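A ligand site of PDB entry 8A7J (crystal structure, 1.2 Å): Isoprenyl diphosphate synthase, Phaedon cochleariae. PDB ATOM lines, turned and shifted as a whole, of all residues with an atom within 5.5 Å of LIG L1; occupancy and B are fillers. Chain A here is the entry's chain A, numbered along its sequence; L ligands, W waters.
Water W1 bridges O3 of LIG L1 (2.7 Å) and OG1 of Thr 52 (3.4 Å). Water W7 lies within hydrogen-bond range of O2 of LIG L1 (2.7 Å) and NZ of Lys 250 (2.8 Å). Water W3 lies within hydrogen-bond range of an oxygen (O6) of LIG L1, the backbone NH (N) of Thr 52 and the backbone NH (N) of Lys 51. Water W5 lies within hydrogen-bond range of O5 of LIG L1 (2.8 Å) and NH1 of Arg 105 (3.0 Å). Water W6 lies within hydrogen-bond range of the side-chain carboxylate (OE1) of Glu 86 (2.7 Å), an oxygen (O7) of LIG L1 (2.8 Å), the backbone NH (N) of Lys 51 (2.9 Å) and the guanidinium group (NH2) of Arg 106 (3.5 Å). Water W2 lies within hydrogen-bond range of the side-chain carboxylate of Asp 236 (2.8 Å), the guanidinium group of Arg 344 (2.9 Å) and an oxygen (O2) of LIG L1 (2.9 Å).
The guanidinium group of Arg 53 is in salt-bridge range of an oxygen (O3) of LIG L1. NE2 of Gln 89 lies within hydrogen-bond range of O7 of LIG L1, at 2.8 Å. NH2 of Arg 106 lies within salt-bridge range of O7 of LIG L1 (2.8 Å). An oxygen (O6) of LIG L1 lies within hydrogen-bond range of the backbone NH (N) of Lys 50, at 2.8 Å. NZ of Lys 50 is in salt-bridge range of O2 of LIG L1 (2.9 Å). OG1 of Thr 194 is in hydrogen-bond range of N2 of LG2 L2 (2.9 Å). The side-chain amino group (NZ) of Lys 250 lies within salt-bridge range of an oxygen (O6) of LG2 L2 (2.8 Å). NH1 of Arg 105 lies within salt-bridge range of O6 of LG2 L2 (2.8 Å). The side-chain amino group (NZ) of Lys 193 is in salt-bridge range of an oxygen (O1) of LG2 L2 (2.7 Å).
The guanidinium group (NH1) of Arg 53 sits close to the side-chain amide nitrogen (NE2) of Gln 89 (3.3 Å). The side-chain amide oxygen of Gln 89 sits at hydrogen-bond distance from the side-chain hydroxyl of Tyr 197. NE2 of Gln 233 sits close to OD2 of Asp 236, at 3.0 Å. OD1 of Asp 236 lies within salt-bridge range of NZ of Lys 250. O of Phe 232 lies within hydrogen-bond range of NH2 of Arg 344, at 3.1 Å. OG1 of Thr 194 is in hydrogen-bond range of OE1 of Gln 233 (2.7 Å). OG1 of Thr 198 lies within hydrogen-bond range of O of Thr 194. The backbone carbonyl oxygen (O) of Gly 49 lies within hydrogen-bond range of the side-chain amino group (NZ) of Lys 51, at 2.8 Å.
Gly 49 touches LIG L1. Thr 194 touches LIG L1. OH of Tyr 197 touches C4 of LIG L1, at 3.4 Å. OG1 of Thr 198 touches C4 of LIG L1 (3.9 Å). Phe 232 touches LIG L1 (CE2 to C5, 3.5 Å). OE1 of Gln 233 touches C5 of LIG L1, 3.8 Å away. Asp 236 touches LIG L1. 11 residues have an atom within 4 Å of LIG L1: Gly 49, Lys 50, Arg 53, Gln 89, Arg 106, Thr 194, Tyr 197, Thr 198, Phe 232, Gln 233 and Asp 236. The nearest printed residue that does not touch LIG L1 is Arg 344 (4.1 Å).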
ATOM      1  N   GLY A  49      -7.938 -14.331 -25.951  1.00  0.00           N
ATOM      2  CA  GLY A  49      -8.460 -14.989 -24.756  1.00  0.00           C
ATOM      3  C   GLY A  49      -9.962 -14.800 -24.622  1.00  0.00           C
ATOM      4  O   GLY A  49     -10.625 -14.298 -25.521  1.00  0.00           O
ATOM      5  N   LYS A  50     -10.471 -15.159 -23.449  1.00  0.00           N
ATOM      6  CA  LYS A  50     -11.924 -15.078 -23.189  1.00  0.00           C
ATOM      7  C   LYS A  50     -12.334 -13.632 -22.918  1.00  0.00           C
ATOM      8  O   LYS A  50     -13.539 -13.324 -23.021  1.00  0.00           O
ATOM      9  CB  LYS A  50     -12.342 -15.965 -22.039  1.00  0.00           C
ATOM     10  CG  LYS A  50     -12.074 -17.450 -22.290  1.00  0.00           C
ATOM     11  CD  LYS A  50     -12.369 -18.302 -21.075  1.00  0.00           C
ATOM     12  CE  LYS A  50     -11.542 -17.980 -19.871  1.00  0.00           C
ATOM     13  NZ  LYS A  50     -10.232 -18.536 -20.116  1.00  0.00           N
ATOM     14  N   LYS A  51     -11.413 -12.774 -22.507  1.00  0.00           N
ATOM     15  CA  LYS A  51     -11.668 -11.333 -22.259  1.00  0.00           C
ATOM     16  C   LYS A  51     -12.599 -11.129 -21.043  1.00  0.00           C
ATOM     17  O   LYS A  51     -13.233 -10.074 -20.950  1.00  0.00           O
ATOM     18  CB  LYS A  51     -12.141 -10.610 -23.530  1.00  0.00           C
ATOM     19  CG  LYS A  51     -11.050 -10.604 -24.585  1.00  0.00           C
ATOM     20  CD  LYS A  51     -11.458 -10.071 -25.933  1.00  0.00           C
ATOM     21  CE  LYS A  51     -12.351 -10.996 -26.703  1.00  0.00           C
ATOM     22  NZ  LYS A  51     -11.613 -12.199 -27.142  1.00  0.00           N
ATOM     23  N   THR A  52     -12.694 -12.081 -20.121  1.00  0.00           N
ATOM     24  CA  THR A  52     -13.575 -11.918 -18.961  1.00  0.00           C
ATOM     25  C   THR A  52     -13.171 -10.708 -18.125  1.00  0.00           C
ATOM     26  O   THR A  52     -14.082 -10.005 -17.647  1.00  0.00           O
ATOM     27  CB  THR A  52     -13.614 -13.192 -18.133  1.00  0.00           C
ATOM     28  OG1 THR A  52     -14.081 -14.229 -18.995  1.00  0.00           O
ATOM     29  CG2 THR A  52     -14.518 -13.116 -16.931  1.00  0.00           C
ATOM     30  N   ARG A  53     -11.884 -10.448 -17.931  1.00  0.00           N
ATOM     31  CA  ARG A  53     -11.483  -9.296 -17.102  1.00  0.00           C
ATOM     32  C   ARG A  53     -11.895  -7.981 -17.771  1.00  0.00           C
ATOM     33  O   ARG A  53     -12.460  -7.100 -17.103  1.00  0.00           O
ATOM     34  CB  ARG A  53      -9.972  -9.276 -16.886  1.00  0.00           C
ATOM     35  CG  ARG A  53      -9.432 -10.464 -16.119  1.00  0.00           C
ATOM     36  CD  ARG A  53      -7.917 -10.601 -16.273  1.00  0.00           C
ATOM     37  NE  ARG A  53      -7.397 -11.815 -15.662  1.00  0.00           N
ATOM     38  CZ  ARG A  53      -7.571 -13.044 -16.132  1.00  0.00           C
ATOM     39  NH1 ARG A  53      -8.230 -13.269 -17.249  1.00  0.00           N
ATOM     40  NH2 ARG A  53      -7.079 -14.079 -15.467  1.00  0.00           N
ATOM     41  N   GLU A  86      -6.675  -6.152 -19.995  1.00  0.00           N
ATOM     42  CA  GLU A  86      -6.260  -7.182 -20.957  1.00  0.00           C
ATOM     43  C   GLU A  86      -4.800  -7.022 -21.390  1.00  0.00           C
ATOM     44  O   GLU A  86      -4.145  -8.054 -21.602  1.00  0.00           O
ATOM     45  CB  GLU A  86      -7.195  -7.241 -22.156  1.00  0.00           C
ATOM     46  CG  GLU A  86      -8.615  -7.675 -21.795  1.00  0.00           C
ATOM     47  CD  GLU A  86      -8.735  -9.104 -21.295  1.00  0.00           C
ATOM     48  OE1 GLU A  86      -7.875  -9.952 -21.668  1.00  0.00           O
ATOM     49  OE2 GLU A  86      -9.717  -9.381 -20.538  1.00  0.00           O
ATOM     50  N   GLN A  89      -2.920  -8.519 -18.456  1.00  0.00           N
ATOM     51  CA  GLN A  89      -3.031  -9.998 -18.581  1.00  0.00           C
ATOM     52  C   GLN A  89      -2.087 -10.485 -19.676  1.00  0.00           C
ATOM     53  O   GLN A  89      -1.352 -11.478 -19.508  1.00  0.00           O
ATOM     54  CB  GLN A  89      -4.479 -10.368 -18.936  1.00  0.00           C
ATOM     55  CG  GLN A  89      -4.712 -11.806 -19.444  1.00  0.00           C
ATOM     56  CD  GLN A  89      -4.621 -12.853 -18.371  1.00  0.00           C
ATOM     57  OE1 GLN A  89      -3.857 -12.683 -17.411  1.00  0.00           O
ATOM     58  NE2 GLN A  89      -5.331 -13.951 -18.557  1.00  0.00           N
ATOM     59  N   LEU A  93       0.965 -13.233 -19.115  1.00  0.00           N
ATOM     60  CA  LEU A  93       0.974 -14.563 -19.740  1.00  0.00           C
ATOM     61  C   LEU A  93       2.246 -14.767 -20.569  1.00  0.00           C
ATOM     62  O   LEU A  93       2.776 -15.884 -20.584  1.00  0.00           O
ATOM     63  CB  LEU A  93      -0.277 -14.848 -20.558  1.00  0.00           C
ATOM     64  CG  LEU A  93      -1.604 -14.730 -19.774  1.00  0.00           C
ATOM     65  CD1 LEU A  93      -2.753 -15.212 -20.677  1.00  0.00           C
ATOM     66  CD2 LEU A  93      -1.568 -15.545 -18.485  1.00  0.00           C
ATOM     67  N   ARG A 105      -0.512 -21.568 -25.663  1.00  0.00           N
ATOM     68  CA  ARG A 105      -1.325 -20.534 -24.974  1.00  0.00           C
ATOM     69  C   ARG A 105      -2.419 -20.125 -25.956  1.00  0.00           C
ATOM     70  O   ARG A 105      -2.116 -19.788 -27.090  1.00  0.00           O
ATOM     71  CB  ARG A 105      -0.443 -19.335 -24.618  1.00  0.00           C
ATOM     72  CG  ARG A 105      -1.207 -18.139 -24.100  1.00  0.00           C
ATOM     73  CD  ARG A 105      -1.908 -18.325 -22.757  1.00  0.00           C
ATOM     74  NE  ARG A 105      -0.939 -18.510 -21.700  1.00  0.00           N
ATOM     75  CZ  ARG A 105      -1.249 -18.761 -20.435  1.00  0.00           C
ATOM     76  NH1 ARG A 105      -2.500 -18.857 -20.059  1.00  0.00           N
ATOM     77  NH2 ARG A 105      -0.292 -18.885 -19.517  1.00  0.00           N
ATOM     78  N   ARG A 106      -3.645 -20.131 -25.514  1.00  0.00           N
ATOM     79  CA  ARG A 106      -4.781 -19.672 -26.327  1.00  0.00           C
ATOM     80  C   ARG A 106      -4.777 -20.380 -27.692  1.00  0.00           C
ATOM     81  O   ARG A 106      -5.151 -19.784 -28.706  1.00  0.00           O
ATOM     82  CB  ARG A 106      -4.798 -18.147 -26.413  1.00  0.00           C
ATOM     83  CG  ARG A 106      -5.058 -17.469 -25.082  1.00  0.00           C
ATOM     84  CD  ARG A 106      -4.788 -15.963 -25.177  1.00  0.00           C
ATOM     85  NE  ARG A 106      -5.116 -15.264 -23.954  1.00  0.00           N
ATOM     86  CZ  ARG A 106      -4.866 -13.978 -23.743  1.00  0.00           C
ATOM     87  NH1 ARG A 106      -4.217 -13.270 -24.666  1.00  0.00           N
ATOM     88  NH2 ARG A 106      -5.220 -13.421 -22.601  1.00  0.00           N
ATOM     89  N   LYS A 193      -0.986 -13.802  -6.871  1.00  0.00           N
ATOM     90  CA  LYS A 193      -0.657 -14.021  -8.291  1.00  0.00           C
ATOM     91  C   LYS A 193      -1.862 -13.896  -9.203  1.00  0.00           C
ATOM     92  O   LYS A 193      -1.664 -13.774 -10.420  1.00  0.00           O
ATOM     93  CB  LYS A 193       0.055 -15.363  -8.534  1.00  0.00           C
ATOM     94  CG  LYS A 193      -0.853 -16.586  -8.576  1.00  0.00           C
ATOM     95  CD  LYS A 193      -0.196 -17.785  -9.167  1.00  0.00           C
ATOM     96  CE  LYS A 193      -1.113 -18.987  -9.157  1.00  0.00           C
ATOM     97  NZ  LYS A 193      -0.501 -20.172  -9.828  1.00  0.00           N
ATOM     98  N   THR A 194      -3.070 -13.965  -8.663  1.00  0.00           N
ATOM     99  CA  THR A 194      -4.294 -14.049  -9.484  1.00  0.00           C
ATOM    100  C   THR A 194      -5.392 -13.091  -9.017  1.00  0.00           C
ATOM    101  O   THR A 194      -5.959 -12.359  -9.851  1.00  0.00           O
ATOM    102  CB  THR A 194      -4.823 -15.479  -9.576  1.00  0.00           C
ATOM    103  OG1 THR A 194      -3.910 -16.167 -10.420  1.00  0.00           O
ATOM    104  CG2 THR A 194      -6.223 -15.531 -10.124  1.00  0.00           C
ATOM    105  N   TYR A 197      -5.374  -8.986  -9.703  1.00  0.00           N
ATOM    106  CA  TYR A 197      -5.433  -8.432 -11.062  1.00  0.00           C
ATOM    107  C   TYR A 197      -6.649  -8.965 -11.816  1.00  0.00           C
ATOM    108  O   TYR A 197      -7.117  -8.310 -12.746  1.00  0.00           O
ATOM    109  CB  TYR A 197      -4.150  -8.660 -11.852  1.00  0.00           C
ATOM    110  CG  TYR A 197      -4.066  -9.950 -12.646  1.00  0.00           C
ATOM    111  CD1 TYR A 197      -3.550 -11.128 -12.113  1.00  0.00           C
ATOM    112  CD2 TYR A 197      -4.433  -9.988 -13.973  1.00  0.00           C
ATOM    113  CE1 TYR A 197      -3.439 -12.286 -12.860  1.00  0.00           C
ATOM    114  CE2 TYR A 197      -4.315 -11.127 -14.743  1.00  0.00           C
ATOM    115  CZ  TYR A 197      -3.813 -12.287 -14.186  1.00  0.00           C
ATOM    116  OH  TYR A 197      -3.672 -13.429 -14.911  1.00  0.00           O
ATOM    117  N   THR A 198      -7.124 -10.155 -11.455  1.00  0.00           N
ATOM    118  CA  THR A 198      -8.189 -10.792 -12.246  1.00  0.00           C
ATOM    119  C   THR A 198      -9.570 -10.297 -11.783  1.00  0.00           C
ATOM    120  O   THR A 198     -10.476 -10.194 -12.624  1.00  0.00           O
ATOM    121  CB  THR A 198      -8.068 -12.319 -12.169  1.00  0.00           C
ATOM    122  OG1 THR A 198      -6.803 -12.706 -12.739  1.00  0.00           O
ATOM    123  CG2 THR A 198      -9.186 -13.043 -12.913  1.00  0.00           C
ATOM    124  N   PHE A 232     -11.527 -19.389  -8.631  1.00  0.00           N
ATOM    125  CA  PHE A 232     -11.109 -19.354 -10.047  1.00  0.00           C
ATOM    126  C   PHE A 232      -9.749 -20.029 -10.253  1.00  0.00           C
ATOM    127  O   PHE A 232      -9.577 -20.749 -11.264  1.00  0.00           O
ATOM    128  CB  PHE A 232     -11.077 -17.884 -10.476  1.00  0.00           C
ATOM    129  CG  PHE A 232     -10.680 -17.674 -11.903  1.00  0.00           C
ATOM    130  CD1 PHE A 232     -11.591 -17.922 -12.918  1.00  0.00           C
ATOM    131  CD2 PHE A 232      -9.408 -17.247 -12.261  1.00  0.00           C
ATOM    132  CE1 PHE A 232     -11.253 -17.684 -14.250  1.00  0.00           C
ATOM    133  CE2 PHE A 232      -9.074 -16.979 -13.572  1.00  0.00           C
ATOM    134  CZ  PHE A 232      -9.982 -17.236 -14.566  1.00  0.00           C
ATOM    135  N   GLN A 233      -8.786 -19.738  -9.398  1.00  0.00           N
ATOM    136  CA  GLN A 233      -7.456 -20.365  -9.523  1.00  0.00           C
ATOM    137  C   GLN A 233      -7.522 -21.859  -9.253  1.00  0.00           C
ATOM    138  O   GLN A 233      -6.752 -22.610  -9.890  1.00  0.00           O
ATOM    139  CB  GLN A 233      -6.431 -19.637  -8.672  1.00  0.00           C
ATOM    140  CG  GLN A 233      -5.012 -20.106  -8.946  1.00  0.00           C
ATOM    141  CD  GLN A 233      -4.548 -19.834 -10.345  1.00  0.00           C
ATOM    142  OE1 GLN A 233      -4.687 -18.714 -10.851  1.00  0.00           O
ATOM    143  NE2 GLN A 233      -3.961 -20.839 -10.987  1.00  0.00           N
ATOM    144  N   ASP A 236      -8.480 -23.286 -12.397  1.00  0.00           N
ATOM    145  CA  ASP A 236      -7.337 -23.263 -13.333  1.00  0.00           C
ATOM    146  C   ASP A 236      -6.426 -24.458 -13.049  1.00  0.00           C
ATOM    147  O   ASP A 236      -5.911 -25.096 -13.998  1.00  0.00           O
ATOM    148  CB  ASP A 236      -6.554 -21.962 -13.214  1.00  0.00           C
ATOM    149  CG  ASP A 236      -5.427 -21.889 -14.220  1.00  0.00           C
ATOM    150  OD1 ASP A 236      -5.770 -21.845 -15.437  1.00  0.00           O
ATOM    151  OD2 ASP A 236      -4.240 -21.887 -13.788  1.00  0.00           O
ATOM    152  N   LYS A 250      -4.235 -24.616 -23.755  1.00  0.00           N
ATOM    153  CA  LYS A 250      -2.913 -24.678 -23.125  1.00  0.00           C
ATOM    154  C   LYS A 250      -2.667 -26.074 -22.595  1.00  0.00           C
ATOM    155  O   LYS A 250      -3.558 -26.741 -22.078  1.00  0.00           O
ATOM    156  CB  LYS A 250      -2.792 -23.590 -22.050  1.00  0.00           C
ATOM    157  CG  LYS A 250      -3.733 -23.716 -20.888  1.00  0.00           C
ATOM    158  CD  LYS A 250      -3.776 -22.427 -20.018  1.00  0.00           C
ATOM    159  CE  LYS A 250      -4.503 -22.669 -18.726  1.00  0.00           C
ATOM    160  NZ  LYS A 250      -4.640 -21.427 -17.934  1.00  0.00           N
ATOM    161  N   ARG A 344     -16.840 -23.960 -15.617  1.00  0.00           N
ATOM    162  CA  ARG A 344     -16.116 -23.719 -16.884  1.00  0.00           C
ATOM    163  C   ARG A 344     -15.152 -24.860 -17.234  1.00  0.00           C
ATOM    164  O   ARG A 344     -14.602 -25.534 -16.347  1.00  0.00           O
ATOM    165  CB  ARG A 344     -15.315 -22.424 -16.804  1.00  0.00           C
ATOM    166  CG  ARG A 344     -14.139 -22.386 -15.864  1.00  0.00           C
ATOM    167  CD  ARG A 344     -13.657 -20.977 -15.619  1.00  0.00           C
ATOM    168  NE  ARG A 344     -12.512 -20.887 -14.751  1.00  0.00           N
ATOM    169  CZ  ARG A 344     -11.245 -20.915 -15.167  1.00  0.00           C
ATOM    170  NH1 ARG A 344     -10.954 -20.988 -16.458  1.00  0.00           N
ATOM    171  NH2 ARG A 344     -10.252 -20.854 -14.290  1.00  0.00           N
ATOM    172  N   ALA A 346     -12.722 -24.093 -19.659  1.00  0.00           N
ATOM    173  CA  ALA A 346     -11.656 -23.309 -20.320  1.00  0.00           C
ATOM    174  C   ALA A 346     -11.505 -21.978 -19.581  1.00  0.00           C
ATOM    175  O   ALA A 346     -10.456 -21.383 -19.703  1.00  0.00           O
ATOM    176  CB  ALA A 346     -11.986 -23.032 -21.767  1.00  0.00           C
ATOM    177  OXT ALA A 346     -12.477 -21.588 -18.858  1.00  0.00           O
HETATM  178  C1  LIG L   1      -5.401 -17.389 -17.167  1.00  0.00           C
HETATM  179  O1  LIG L   1      -6.602 -16.568 -17.217  1.00  0.00           O
HETATM  180  C2  LIG L   1      -4.596 -17.023 -15.947  1.00  0.00           C
HETATM  181  C3  LIG L   1      -5.316 -17.175 -14.622  1.00  0.00           C
HETATM  182  C4  LIG L   1      -5.284 -16.209 -13.723  1.00  0.00           C
HETATM  183  C5  LIG L   1      -5.975 -18.471 -14.413  1.00  0.00           C
HETATM  184  P1  LIG L   1      -7.808 -16.940 -18.180  1.00  0.00           P
HETATM  185  O2  LIG L   1      -8.159 -18.375 -18.028  1.00  0.00           O
HETATM  186  O3  LIG L   1      -8.874 -15.926 -17.909  1.00  0.00           O
HETATM  187  O4  LIG L   1      -7.164 -16.766 -19.603  1.00  0.00           O
HETATM  188  P2  LIG L   1      -7.520 -15.888 -20.965  1.00  0.00           P
HETATM  189  O5  LIG L   1      -6.756 -16.606 -22.047  1.00  0.00           O
HETATM  190  O6  LIG L   1      -9.016 -15.984 -21.145  1.00  0.00           O
HETATM  191  O7  LIG L   1      -7.050 -14.500 -20.726  1.00  0.00           O
HETATM  192  O1  LG2 L   2      -0.370 -19.429 -12.405  1.00  0.00           O
HETATM  193  P1  LG2 L   2      -0.422 -20.270 -13.669  1.00  0.00           P
HETATM  194  O2  LG2 L   2       0.965 -20.359 -14.372  1.00  0.00           O
HETATM  195  O3  LG2 L   2      -1.050 -21.651 -13.439  1.00  0.00           O
HETATM  196  C1  LG2 L   2      -1.522 -19.457 -14.911  1.00  0.00           C
HETATM  197  P2  LG2 L   2      -1.664 -20.435 -16.466  1.00  0.00           P
HETATM  198  O4  LG2 L   2      -2.331 -21.750 -16.065  1.00  0.00           O
HETATM  199  O5  LG2 L   2      -0.286 -20.635 -16.999  1.00  0.00           O
HETATM  200  O6  LG2 L   2      -2.551 -19.616 -17.392  1.00  0.00           O
HETATM  201  O7  LG2 L   2      -2.849 -19.364 -14.331  1.00  0.00           O
HETATM  202  C2  LG2 L   2      -1.082 -18.026 -15.236  1.00  0.00           C
HETATM  203  N1  LG2 L   2      -1.059 -17.113 -14.081  1.00  0.00           N
HETATM  204  C3  LG2 L   2      -2.068 -16.845 -13.215  1.00  0.00           C
HETATM  205  N2  LG2 L   2      -1.682 -15.971 -12.323  1.00  0.00           N
HETATM  206  C4  LG2 L   2      -0.402 -15.634 -12.605  1.00  0.00           C
HETATM  207  C5  LG2 L   2      -0.016 -16.294 -13.715  1.00  0.00           C
HETATM  208  O   HOH W   1     -11.484 -15.639 -17.295  1.00  0.00           O
HETATM  209  O   HOH W   2      -8.112 -20.626 -16.245  1.00  0.00           O
HETATM  210  O   HOH W   3     -10.515 -14.148 -19.767  1.00  0.00           O
HETATM  211  O   HOH W   4      -8.359 -18.457 -23.338  1.00  0.00           O
HETATM  212  O   HOH W   5      -5.129 -18.753 -21.397  1.00  0.00           O
HETATM  213  O   HOH W   6      -8.533 -12.553 -22.092  1.00  0.00           O
HETATM  214  O   HOH W   7      -6.591 -20.091 -19.460  1.00  0.00           O
